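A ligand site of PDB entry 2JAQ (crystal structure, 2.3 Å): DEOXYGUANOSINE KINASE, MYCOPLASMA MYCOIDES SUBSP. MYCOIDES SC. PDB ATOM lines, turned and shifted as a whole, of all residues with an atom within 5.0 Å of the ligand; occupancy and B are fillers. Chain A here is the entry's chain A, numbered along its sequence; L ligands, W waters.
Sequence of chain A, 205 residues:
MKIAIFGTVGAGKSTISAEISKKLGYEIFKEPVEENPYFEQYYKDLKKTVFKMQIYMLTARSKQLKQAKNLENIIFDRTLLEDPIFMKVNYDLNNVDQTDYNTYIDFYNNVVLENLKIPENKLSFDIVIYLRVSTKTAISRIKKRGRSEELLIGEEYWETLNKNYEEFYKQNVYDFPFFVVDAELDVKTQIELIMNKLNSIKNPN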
ATOM      1  N   GLY A   7      12.330 -14.659 -17.697  1.00  0.00           N
ATOM      2  CA  GLY A   7      12.871 -15.134 -16.442  1.00  0.00           C
ATOM      3  C   GLY A   7      11.903 -15.066 -15.286  1.00  0.00           C
ATOM      4  O   GLY A   7      10.899 -14.362 -15.339  1.00  0.00           O
ATOM      5  N   THR A   8      12.237 -15.797 -14.241  1.00  0.00           N
ATOM      6  CA  THR A   8      11.399 -15.909 -13.054  1.00  0.00           C
ATOM      7  C   THR A   8      11.345 -14.606 -12.240  1.00  0.00           C
ATOM      8  O   THR A   8      12.037 -13.632 -12.568  1.00  0.00           O
ATOM      9  CB  THR A   8      11.871 -17.126 -12.166  1.00  0.00           C
ATOM     10  OG1 THR A   8      10.878 -17.383 -11.178  1.00  0.00           O
ATOM     11  CG2 THR A   8      13.203 -16.853 -11.484  1.00  0.00           C
ATOM     12  N   VAL A   9      10.504 -14.598 -11.205  1.00  0.00           N
ATOM     13  CA  VAL A   9      10.405 -13.470 -10.281  1.00  0.00           C
ATOM     14  C   VAL A   9      11.739 -13.236  -9.554  1.00  0.00           C
ATOM     15  O   VAL A   9      12.286 -14.142  -8.909  1.00  0.00           O
ATOM     16  CB  VAL A   9       9.251 -13.681  -9.264  1.00  0.00           C
ATOM     17  CG1 VAL A   9       9.122 -12.502  -8.304  1.00  0.00           C
ATOM     18  CG2 VAL A   9       7.933 -13.914  -9.998  1.00  0.00           C
ATOM     19  N   GLY A  10      12.285 -12.022  -9.686  1.00  0.00           N
ATOM     20  CA  GLY A  10      13.537 -11.660  -9.033  1.00  0.00           C
ATOM     21  C   GLY A  10      14.753 -11.943  -9.889  1.00  0.00           C
ATOM     22  O   GLY A  10      15.891 -11.795  -9.420  1.00  0.00           O
ATOM     23  N   ALA A  11      14.532 -12.345 -11.147  1.00  0.00           N
ATOM     24  CA  ALA A  11      15.595 -12.546 -12.144  1.00  0.00           C
ATOM     25  C   ALA A  11      16.276 -11.247 -12.563  1.00  0.00           C
ATOM     26  O   ALA A  11      17.431 -11.248 -13.008  1.00  0.00           O
ATOM     27  CB  ALA A  11      15.046 -13.250 -13.377  1.00  0.00           C
ATOM     28  N   GLY A  12      15.553 -10.129 -12.418  1.00  0.00           N
ATOM     29  CA  GLY A  12      16.089  -8.811 -12.791  1.00  0.00           C
ATOM     30  C   GLY A  12      15.667  -8.323 -14.165  1.00  0.00           C
ATOM     31  O   GLY A  12      16.365  -7.523 -14.790  1.00  0.00           O
ATOM     32  N   LYS A  13      14.514  -8.803 -14.634  1.00  0.00           N
ATOM     33  CA  LYS A  13      13.992  -8.444 -15.962  1.00  0.00           C
ATOM     34  C   LYS A  13      13.796  -6.935 -16.157  1.00  0.00           C
ATOM     35  O   LYS A  13      14.162  -6.389 -17.207  1.00  0.00           O
ATOM     36  CB  LYS A  13      12.682  -9.172 -16.256  1.00  0.00           C
ATOM     37  CG  LYS A  13      12.821 -10.696 -16.410  1.00  0.00           C
ATOM     38  CD  LYS A  13      11.502 -11.363 -16.817  1.00  0.00           C
ATOM     39  CE  LYS A  13      10.387 -11.102 -15.818  1.00  0.00           C
ATOM     40  NZ  LYS A  13      10.711 -11.583 -14.453  1.00  0.00           N
ATOM     41  N   SER A  14      13.225  -6.263 -15.167  1.00  0.00           N
ATOM     42  CA  SER A  14      12.908  -4.847 -15.375  1.00  0.00           C
ATOM     43  C   SER A  14      14.167  -3.971 -15.313  1.00  0.00           C
ATOM     44  O   SER A  14      14.290  -2.993 -16.063  1.00  0.00           O
ATOM     45  CB  SER A  14      11.761  -4.371 -14.453  1.00  0.00           C
ATOM     46  OG  SER A  14      12.243  -4.007 -13.180  1.00  0.00           O
ATOM     47  N   THR A  15      15.104  -4.367 -14.468  1.00  0.00           N
ATOM     48  CA  THR A  15      16.422  -3.732 -14.412  1.00  0.00           C
ATOM     49  C   THR A  15      17.185  -3.882 -15.743  1.00  0.00           C
ATOM     50  O   THR A  15      17.657  -2.895 -16.313  1.00  0.00           O
ATOM     51  CB  THR A  15      17.258  -4.318 -13.242  1.00  0.00           C
ATOM     52  OG1 THR A  15      16.527  -4.138 -12.023  1.00  0.00           O
ATOM     53  CG2 THR A  15      18.649  -3.633 -13.129  1.00  0.00           C
ATOM     54  N   LYS A  30       6.057  -3.076 -20.580  1.00  0.00           N
ATOM     55  CA  LYS A  30       5.893  -3.480 -19.197  1.00  0.00           C
ATOM     56  C   LYS A  30       4.427  -3.709 -18.897  1.00  0.00           C
ATOM     57  O   LYS A  30       3.544  -3.123 -19.523  1.00  0.00           O
ATOM     58  CB  LYS A  30       6.418  -2.391 -18.264  1.00  0.00           C
ATOM     59  CG  LYS A  30       7.830  -2.616 -17.742  1.00  0.00           C
ATOM     60  CD  LYS A  30       7.996  -2.160 -16.286  1.00  0.00           C
ATOM     61  CE  LYS A  30       7.340  -3.132 -15.282  1.00  0.00           C
ATOM     62  NZ  LYS A  30       8.134  -4.384 -15.033  1.00  0.00           N
ATOM     63  N   GLU A  31       4.170  -4.595 -17.937  1.00  0.00           N
ATOM     64  CA  GLU A  31       2.851  -4.756 -17.351  1.00  0.00           C
ATOM     65  C   GLU A  31       2.979  -4.414 -15.865  1.00  0.00           C
ATOM     66  O   GLU A  31       3.392  -5.255 -15.057  1.00  0.00           O
ATOM     67  CB  GLU A  31       2.332  -6.176 -17.570  1.00  0.00           C
ATOM     68  CG  GLU A  31       0.829  -6.250 -17.798  1.00  0.00           C
ATOM     69  CD  GLU A  31       0.354  -5.479 -19.030  1.00  0.00           C
ATOM     70  OE1 GLU A  31       0.820  -4.347 -19.269  1.00  0.00           O
ATOM     71  OE2 GLU A  31      -0.504  -6.001 -19.769  1.00  0.00           O
ATOM     72  N   VAL A  33       2.771  -3.864 -12.080  1.00  0.00           N
ATOM     73  CA  VAL A  33       2.140  -4.591 -10.978  1.00  0.00           C
ATOM     74  C   VAL A  33       1.185  -3.719 -10.152  1.00  0.00           C
ATOM     75  O   VAL A  33       0.236  -4.234  -9.552  1.00  0.00           O
ATOM     76  CB  VAL A  33       3.222  -5.313 -10.098  1.00  0.00           C
ATOM     77  CG1 VAL A  33       3.279  -4.754  -8.665  1.00  0.00           C
ATOM     78  CG2 VAL A  33       3.011  -6.801 -10.109  1.00  0.00           C
ATOM     79  N   PHE A  39      -3.458  -8.037  -7.601  1.00  0.00           N
ATOM     80  CA  PHE A  39      -2.159  -8.271  -6.980  1.00  0.00           C
ATOM     81  C   PHE A  39      -2.171  -8.200  -5.455  1.00  0.00           C
ATOM     82  O   PHE A  39      -1.581  -9.069  -4.792  1.00  0.00           O
ATOM     83  CB  PHE A  39      -1.107  -7.308  -7.568  1.00  0.00           C
ATOM     84  CG  PHE A  39       0.299  -7.666  -7.232  1.00  0.00           C
ATOM     85  CD1 PHE A  39       0.883  -8.831  -7.728  1.00  0.00           C
ATOM     86  CD2 PHE A  39       1.068  -6.840  -6.406  1.00  0.00           C
ATOM     87  CE1 PHE A  39       2.202  -9.172  -7.417  1.00  0.00           C
ATOM     88  CE2 PHE A  39       2.393  -7.163  -6.080  1.00  0.00           C
ATOM     89  CZ  PHE A  39       2.958  -8.331  -6.592  1.00  0.00           C
ATOM     90  N   TYR A  42      -3.794 -11.460  -4.247  1.00  0.00           N
ATOM     91  CA  TYR A  42      -3.343 -12.644  -4.963  1.00  0.00           C
ATOM     92  C   TYR A  42      -2.640 -13.672  -4.060  1.00  0.00           C
ATOM     93  O   TYR A  42      -3.072 -14.825  -3.965  1.00  0.00           O
ATOM     94  CB  TYR A  42      -2.444 -12.212  -6.133  1.00  0.00           C
ATOM     95  CG  TYR A  42      -1.876 -13.329  -6.977  1.00  0.00           C
ATOM     96  CD1 TYR A  42      -2.712 -14.273  -7.581  1.00  0.00           C
ATOM     97  CD2 TYR A  42      -0.506 -13.400  -7.215  1.00  0.00           C
ATOM     98  CE1 TYR A  42      -2.181 -15.292  -8.371  1.00  0.00           C
ATOM     99  CE2 TYR A  42       0.025 -14.405  -8.002  1.00  0.00           C
ATOM    100  CZ  TYR A  42      -0.808 -15.347  -8.583  1.00  0.00           C
ATOM    101  OH  TYR A  42      -0.263 -16.339  -9.364  1.00  0.00           O
ATOM    102  N   TYR A  43      -1.578 -13.237  -3.401  1.00  0.00           N
ATOM    103  CA  TYR A  43      -0.724 -14.142  -2.628  1.00  0.00           C
ATOM    104  C   TYR A  43      -1.311 -14.584  -1.279  1.00  0.00           C
ATOM    105  O   TYR A  43      -0.871 -15.595  -0.730  1.00  0.00           O
ATOM    106  CB  TYR A  43       0.676 -13.545  -2.448  1.00  0.00           C
ATOM    107  CG  TYR A  43       1.508 -13.570  -3.706  1.00  0.00           C
ATOM    108  CD1 TYR A  43       1.802 -12.404  -4.391  1.00  0.00           C
ATOM    109  CD2 TYR A  43       1.990 -14.783  -4.224  1.00  0.00           C
ATOM    110  CE1 TYR A  43       2.564 -12.425  -5.550  1.00  0.00           C
ATOM    111  CE2 TYR A  43       2.744 -14.813  -5.375  1.00  0.00           C
ATOM    112  CZ  TYR A  43       3.027 -13.630  -6.038  1.00  0.00           C
ATOM    113  OH  TYR A  43       3.772 -13.654  -7.180  1.00  0.00           O
ATOM    114  N   MET A  53      -6.627 -14.081 -11.642  1.00  0.00           N
ATOM    115  CA  MET A  53      -5.387 -13.373 -11.899  1.00  0.00           C
ATOM    116  C   MET A  53      -4.788 -13.746 -13.270  1.00  0.00           C
ATOM    117  O   MET A  53      -4.385 -12.882 -14.026  1.00  0.00           O
ATOM    118  CB  MET A  53      -4.372 -13.628 -10.790  1.00  0.00           C
ATOM    119  CG  MET A  53      -2.957 -13.177 -11.138  1.00  0.00           C
ATOM    120  SD  MET A  53      -2.854 -11.383 -11.210  1.00  0.00           S
ATOM    121  CE  MET A  53      -2.278 -11.025  -9.563  1.00  0.00           C
ATOM    122  N   GLN A  54      -4.763 -15.046 -13.558  1.00  0.00           N
ATOM    123  CA  GLN A  54      -4.103 -15.529 -14.772  1.00  0.00           C
ATOM    124  C   GLN A  54      -4.866 -15.195 -16.062  1.00  0.00           C
ATOM    125  O   GLN A  54      -4.253 -15.045 -17.112  1.00  0.00           O
ATOM    126  CB  GLN A  54      -3.752 -17.006 -14.652  1.00  0.00           C
ATOM    127  CG  GLN A  54      -2.757 -17.319 -13.507  1.00  0.00           C
ATOM    128  CD  GLN A  54      -1.407 -16.625 -13.661  1.00  0.00           C
ATOM    129  OE1 GLN A  54      -0.932 -16.394 -14.785  1.00  0.00           O
ATOM    130  NE2 GLN A  54      -0.776 -16.285 -12.539  1.00  0.00           N
ATOM    131  N   MET A  57      -4.040 -11.586 -16.572  1.00  0.00           N
ATOM    132  CA  MET A  57      -2.703 -11.503 -17.170  1.00  0.00           C
ATOM    133  C   MET A  57      -2.753 -11.682 -18.689  1.00  0.00           C
ATOM    134  O   MET A  57      -2.165 -10.883 -19.420  1.00  0.00           O
ATOM    135  CB  MET A  57      -1.738 -12.508 -16.530  1.00  0.00           C
ATOM    136  CG  MET A  57      -1.382 -12.259 -15.068  1.00  0.00           C
ATOM    137  SD  MET A  57      -0.798 -10.600 -14.629  1.00  0.00           S
ATOM    138  CE  MET A  57       0.417 -10.275 -15.911  1.00  0.00           C
ATOM    139  N   ARG A  61      -1.809  -8.568 -21.364  1.00  0.00           N
ATOM    140  CA  ARG A  61      -0.721  -8.828 -22.295  1.00  0.00           C
ATOM    141  C   ARG A  61      -1.193  -8.767 -23.759  1.00  0.00           C
ATOM    142  O   ARG A  61      -0.432  -8.345 -24.626  1.00  0.00           O
ATOM    143  CB  ARG A  61      -0.073 -10.183 -21.973  1.00  0.00           C
ATOM    144  CG  ARG A  61       1.389 -10.327 -22.425  1.00  0.00           C
ATOM    145  CD  ARG A  61       2.381  -9.681 -21.455  1.00  0.00           C
ATOM    146  NE  ARG A  61       2.426 -10.352 -20.157  1.00  0.00           N
ATOM    147  CZ  ARG A  61       3.151  -9.955 -19.117  1.00  0.00           C
ATOM    148  NH1 ARG A  61       3.934  -8.881 -19.197  1.00  0.00           N
ATOM    149  NH2 ARG A  61       3.110 -10.643 -17.987  1.00  0.00           N
ATOM    150  N   ARG A  78       9.162  -9.459 -19.739  1.00  0.00           N
ATOM    151  CA  ARG A  78       8.299 -10.655 -19.681  1.00  0.00           C
ATOM    152  C   ARG A  78       7.338 -10.724 -20.878  1.00  0.00           C
ATOM    153  O   ARG A  78       6.884  -9.700 -21.386  1.00  0.00           O
ATOM    154  CB  ARG A  78       7.588 -10.821 -18.311  1.00  0.00           C
ATOM    155  CG  ARG A  78       6.521 -11.943 -18.249  1.00  0.00           C
ATOM    156  CD  ARG A  78       6.667 -12.843 -17.019  1.00  0.00           C
ATOM    157  NE  ARG A  78       6.417 -12.135 -15.766  1.00  0.00           N
ATOM    158  CZ  ARG A  78       7.017 -12.410 -14.612  1.00  0.00           C
ATOM    159  NH1 ARG A  78       7.924 -13.386 -14.521  1.00  0.00           N
ATOM    160  NH2 ARG A  78       6.708 -11.696 -13.537  1.00  0.00           N
ATOM    161  N   GLU A  82       5.246 -16.702 -21.090  1.00  0.00           N
ATOM    162  CA  GLU A  82       5.582 -16.986 -19.701  1.00  0.00           C
ATOM    163  C   GLU A  82       4.381 -17.131 -18.785  1.00  0.00           C
ATOM    164  O   GLU A  82       4.464 -17.815 -17.763  1.00  0.00           O
ATOM    165  CB  GLU A  82       6.536 -15.911 -19.160  1.00  0.00           C
ATOM    166  CG  GLU A  82       7.935 -16.055 -19.699  1.00  0.00           C
ATOM    167  CD  GLU A  82       8.786 -14.822 -19.491  1.00  0.00           C
ATOM    168  OE1 GLU A  82       9.329 -14.626 -18.386  1.00  0.00           O
ATOM    169  OE2 GLU A  82       8.946 -14.060 -20.455  1.00  0.00           O
ATOM    170  N   ASP A  83       3.283 -16.476 -19.119  1.00  0.00           N
ATOM    171  CA  ASP A  83       2.082 -16.538 -18.280  1.00  0.00           C
ATOM    172  C   ASP A  83       1.577 -17.946 -17.961  1.00  0.00           C
ATOM    173  O   ASP A  83       1.299 -18.232 -16.797  1.00  0.00           O
ATOM    174  CB  ASP A  83       0.968 -15.652 -18.840  1.00  0.00           C
ATOM    175  CG  ASP A  83       1.333 -14.188 -18.853  1.00  0.00           C
ATOM    176  OD1 ASP A  83       1.826 -13.662 -17.825  1.00  0.00           O
ATOM    177  OD2 ASP A  83       1.120 -13.552 -19.892  1.00  0.00           O
ATOM    178  N   PHE A  86       3.083 -19.761 -14.904  1.00  0.00           N
ATOM    179  CA  PHE A  86       2.511 -19.470 -13.597  1.00  0.00           C
ATOM    180  C   PHE A  86       1.257 -20.284 -13.281  1.00  0.00           C
ATOM    181  O   PHE A  86       1.019 -20.627 -12.130  1.00  0.00           O
ATOM    182  CB  PHE A  86       2.243 -17.978 -13.467  1.00  0.00           C
ATOM    183  CG  PHE A  86       3.478 -17.166 -13.308  1.00  0.00           C
ATOM    184  CD1 PHE A  86       4.286 -16.870 -14.400  1.00  0.00           C
ATOM    185  CD2 PHE A  86       3.865 -16.698 -12.054  1.00  0.00           C
ATOM    186  CE1 PHE A  86       5.451 -16.118 -14.248  1.00  0.00           C
ATOM    187  CE2 PHE A  86       5.008 -15.940 -11.894  1.00  0.00           C
ATOM    188  CZ  PHE A  86       5.808 -15.650 -12.990  1.00  0.00           C
ATOM    189  N   ARG A 145      13.574  -5.796  -2.769  1.00  0.00           N
ATOM    190  CA  ARG A 145      12.540  -4.985  -3.401  1.00  0.00           C
ATOM    191  C   ARG A 145      11.442  -4.656  -2.385  1.00  0.00           C
ATOM    192  O   ARG A 145      10.941  -3.526  -2.338  1.00  0.00           O
ATOM    193  CB  ARG A 145      11.974  -5.703  -4.631  1.00  0.00           C
ATOM    194  CG  ARG A 145      10.899  -4.924  -5.404  1.00  0.00           C
ATOM    195  CD  ARG A 145      10.584  -5.593  -6.747  1.00  0.00           C
ATOM    196  NE  ARG A 145      10.205  -7.006  -6.601  1.00  0.00           N
ATOM    197  CZ  ARG A 145      10.269  -7.910  -7.581  1.00  0.00           C
ATOM    198  NH1 ARG A 145       9.902  -9.168  -7.348  1.00  0.00           N
ATOM    199  NH2 ARG A 145      10.684  -7.557  -8.786  1.00  0.00           N
ATOM    200  N   ARG A 147       8.241  -5.851  -1.860  1.00  0.00           N
ATOM    201  CA  ARG A 147       6.793  -5.997  -2.102  1.00  0.00           C
ATOM    202  C   ARG A 147       6.167  -6.879  -1.021  1.00  0.00           C
ATOM    203  O   ARG A 147       6.391  -8.093  -0.988  1.00  0.00           O
ATOM    204  CB  ARG A 147       6.487  -6.578  -3.488  1.00  0.00           C
ATOM    205  CG  ARG A 147       5.900  -5.605  -4.493  1.00  0.00           C
ATOM    206  CD  ARG A 147       6.785  -5.371  -5.718  1.00  0.00           C
ATOM    207  NE  ARG A 147       6.854  -6.539  -6.584  1.00  0.00           N
ATOM    208  CZ  ARG A 147       7.107  -6.511  -7.891  1.00  0.00           C
ATOM    209  NH1 ARG A 147       7.291  -5.362  -8.541  1.00  0.00           N
ATOM    210  NH2 ARG A 147       7.173  -7.647  -8.574  1.00  0.00           N
ATOM    211  N   GLU A 150       4.525 -10.206  -2.116  1.00  0.00           N
ATOM    212  CA  GLU A 150       5.446 -11.292  -2.451  1.00  0.00           C
ATOM    213  C   GLU A 150       6.122 -11.914  -1.218  1.00  0.00           C
ATOM    214  O   GLU A 150       6.535 -13.081  -1.240  1.00  0.00           O
ATOM    215  CB  GLU A 150       6.480 -10.814  -3.469  1.00  0.00           C
ATOM    216  CG  GLU A 150       5.864 -10.482  -4.812  1.00  0.00           C
ATOM    217  CD  GLU A 150       6.819  -9.782  -5.768  1.00  0.00           C
ATOM    218  OE1 GLU A 150       7.963  -9.454  -5.365  1.00  0.00           O
ATOM    219  OE2 GLU A 150       6.410  -9.566  -6.926  1.00  0.00           O
ATOM    220  N   TYR A 157       7.061 -22.106  -3.290  1.00  0.00           N
ATOM    221  CA  TYR A 157       6.476 -21.432  -4.451  1.00  0.00           C
ATOM    222  C   TYR A 157       7.552 -20.957  -5.429  1.00  0.00           C
ATOM    223  O   TYR A 157       7.497 -21.295  -6.617  1.00  0.00           O
ATOM    224  CB  TYR A 157       5.580 -20.260  -4.019  1.00  0.00           C
ATOM    225  CG  TYR A 157       4.820 -19.634  -5.186  1.00  0.00           C
ATOM    226  CD1 TYR A 157       3.631 -20.199  -5.659  1.00  0.00           C
ATOM    227  CD2 TYR A 157       5.314 -18.494  -5.834  1.00  0.00           C
ATOM    228  CE1 TYR A 157       2.954 -19.649  -6.730  1.00  0.00           C
ATOM    229  CE2 TYR A 157       4.639 -17.928  -6.911  1.00  0.00           C
ATOM    230  CZ  TYR A 157       3.458 -18.514  -7.356  1.00  0.00           C
ATOM    231  OH  TYR A 157       2.771 -17.973  -8.420  1.00  0.00           O
ATOM    232  N   TRP A 158       8.516 -20.178  -4.927  1.00  0.00           N
ATOM    233  CA  TRP A 158       9.609 -19.666  -5.747  1.00  0.00           C
ATOM    234  C   TRP A 158      10.441 -20.768  -6.418  1.00  0.00           C
ATOM    235  O   TRP A 158      10.771 -20.676  -7.602  1.00  0.00           O
ATOM    236  CB  TRP A 158      10.499 -18.706  -4.931  1.00  0.00           C
ATOM    237  CG  TRP A 158       9.775 -17.492  -4.360  1.00  0.00           C
ATOM    238  CD1 TRP A 158       9.852 -17.031  -3.079  1.00  0.00           C
ATOM    239  CD2 TRP A 158       8.868 -16.595  -5.052  1.00  0.00           C
ATOM    240  NE1 TRP A 158       9.070 -15.911  -2.926  1.00  0.00           N
ATOM    241  CE2 TRP A 158       8.456 -15.622  -4.111  1.00  0.00           C
ATOM    242  CE3 TRP A 158       8.381 -16.524  -6.360  1.00  0.00           C
ATOM    243  CZ2 TRP A 158       7.573 -14.579  -4.444  1.00  0.00           C
ATOM    244  CZ3 TRP A 158       7.489 -15.489  -6.687  1.00  0.00           C
ATOM    245  CH2 TRP A 158       7.095 -14.541  -5.737  1.00  0.00           C
HETATM  246  N1  LIG L   1       2.763 -12.941 -12.094  1.00  0.00           N
HETATM  247  C1  LIG L   1       1.890 -14.054 -12.021  1.00  0.00           C
HETATM  248  N2  LIG L   1       1.462 -14.641 -13.152  1.00  0.00           N
HETATM  249  C2  LIG L   1       1.845 -14.183 -14.363  1.00  0.00           C
HETATM  250  C3  LIG L   1       2.699 -13.085 -14.464  1.00  0.00           C
HETATM  251  C4  LIG L   1       3.151 -12.466 -13.290  1.00  0.00           C
HETATM  252  O1  LIG L   1       1.521 -14.498 -10.908  1.00  0.00           O
HETATM  253  N3  LIG L   1       1.377 -14.819 -15.460  1.00  0.00           N
HETATM  254  C5  LIG L   1       3.168 -12.312 -10.823  1.00  0.00           C
HETATM  255  C6  LIG L   1       4.562 -12.685 -10.315  1.00  0.00           C
HETATM  256  C7  LIG L   1       5.145 -11.375  -9.804  1.00  0.00           C
HETATM  257  C8  LIG L   1       4.279 -10.297 -10.438  1.00  0.00           C
HETATM  258  O2  LIG L   1       3.112 -10.894 -10.997  1.00  0.00           O
HETATM  259  O3  LIG L   1       5.006 -11.240  -8.375  1.00  0.00           O
HETATM  260  C9  LIG L   1       5.032  -9.648 -11.573  1.00  0.00           C
HETATM  261  O4  LIG L   1       5.774  -8.545 -11.081  1.00  0.00           O
HETATM  262  P1  LIG L   1       6.811  -7.890 -12.113  1.00  0.00           P
HETATM  263  O5  LIG L   1       7.635  -6.867 -11.370  1.00  0.00           O
HETATM  264  O6  LIG L   1       6.067  -7.513 -13.370  1.00  0.00           O
HETATM  265  O7  LIG L   1       7.717  -9.146 -12.560  1.00  0.00           O
HETATM  266  P2  LIG L   1       9.013  -9.692 -11.807  1.00  0.00           P
HETATM  267  O8  LIG L   1       9.060 -11.114 -12.303  1.00  0.00           O
HETATM  268  O9  LIG L   1       8.862  -9.368 -10.342  1.00  0.00           O
HETATM  269  O10 LIG L   1      10.238  -8.814 -12.471  1.00  0.00           O
HETATM  270  P3  LIG L   1      11.838  -8.909 -12.153  1.00  0.00           P
HETATM  271  O11 LIG L   1      11.903  -9.234 -10.685  1.00  0.00           O
HETATM  272  O12 LIG L   1      12.340  -7.542 -12.512  1.00  0.00           O
HETATM  273  O13 LIG L   1      12.416  -9.991 -13.030  1.00  0.00           O
HETATM  274  O   HOH W   1       9.945  -5.983 -12.034  1.00  0.00           O
HETATM  275  O   HOH W   2       3.640 -15.681  -8.978  1.00  0.00           O
HETATM  276  O   HOH W   3       2.818  -7.437 -13.841  1.00  0.00           O
HETATM  277  O   HOH W   4      14.527  -5.981 -12.142  1.00  0.00           O
HETATM  278  O   HOH W   5      14.467  -8.282  -9.402  1.00  0.00           O
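NZ of Lys 13 is in salt-bridge range of O13 of the ligand (2.7 Å).
An oxygen (O11) of the ligand is in salt-bridge range of the guanidinium group (NH2) of Arg 145 (2.8 Å).
A nitrogen (N3) of the ligand is in hydrogen-bond range of the side-chain carboxylate of Asp 83 (2.7 Å).
An oxygen (O13) of the ligand is in hydrogen-bond range of the backbone NH of Lys 13, at 2.9 Å.
The side-chain hydroxyl (OH) of Tyr 42 sits at hydrogen-bond distance from an oxygen (O1) of the ligand, at 3.0 Å.
OH of Tyr 43 sits at hydrogen-bond distance from O3 of the ligand (3.0 Å).
An oxygen (O8) of the ligand lies within salt-bridge range of the guanidinium group (NH2) of Arg 78 (2.7 Å).
The guanidinium group of Arg 147 is in salt-bridge range of an oxygen (O5) of the ligand, 2.9 Å away.
The backbone NH (N) of Gly 10 is in hydrogen-bond range of an oxygen (O11) of the ligand.
O13 of the ligand is in hydrogen-bond range of N of Gly 12, at 3.2 Å.
The side-chain carboxylate (OE2) of Glu 150 lies within hydrogen-bond range of an oxygen (O3) of the ligand.
The backbone NH of Ser 14 lies within hydrogen-bond range of an oxygen (O12) of the ligand (3.1 Å).
A nitrogen (N2) of the ligand sits at hydrogen-bond distance from the side-chain amide nitrogen (NE2) of Gln 54 (2.8 Å).
The side-chain hydroxyl (OH) of Tyr 42 lies within hydrogen-bond range of the side-chain amide nitrogen (NE2) of Gln 54 (3.2 Å).
OE2 of Glu 150 lies within salt-bridge range of NH2 of Arg 147, at 2.6 Å.
The side-chain carboxylate of Glu 150 lies within salt-bridge range of the guanidinium group of Arg 145 (2.8 Å).
NZ of Lys 13 lies within hydrogen-bond range of O of Gly 7, at 2.9 Å.
OE2 of Glu 31 lies within hydrogen-bond range of N of Arg 61, 3.3 Å away.
The guanidinium group of Arg 78 lies within hydrogen-bond range of the backbone carbonyl oxygen of Gly 7, at 3.2 Å.
The side-chain amino group (NZ) of Lys 13 is in hydrogen-bond range of the backbone carbonyl oxygen (O) of Thr 8, at 3.1 Å.
NH2 of Arg 61 is in salt-bridge range of OD1 of Asp 83 (3.3 Å).
Water W1 lies within hydrogen-bond range of O5 of the ligand (2.6 Å) and OG of Ser 14 (3.2 Å).
Water W4 lies within hydrogen-bond range of an oxygen (O12) of the ligand (2.7 Å), the side-chain hydroxyl (OG1) of Thr 15 (2.7 Å) and the side-chain hydroxyl (OG) of Ser 14 (3.2 Å).
Water W2 lies within hydrogen-bond range of OH of Tyr 157, OH of Tyr 43 and O1 of the ligand.
Water W3 bridges the backbone carbonyl oxygen of Glu 31 (2.6 Å) and an oxygen (O6) of the ligand (3.3 Å).
Residues that only touch the ligand: Thr 8, Val 9, Ala 11, Glu 31, Val 33, Phe 39, Met 57 and Phe 86.
20 residues have an atom within 4 Å of the ligand: Thr 8, Val 9, Gly 10, Ala 11, Gly 12, Lys 13, Ser 14, Glu 31, Val 33, Phe 39, Tyr 42, Tyr 43, Gln 54, Met 57, Arg 78, Asp 83, Phe 86, Arg 145, Arg 147 and Glu 150.
The nearest printed residue that does not touch the ligand is Lys 30 (4.1 Å).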
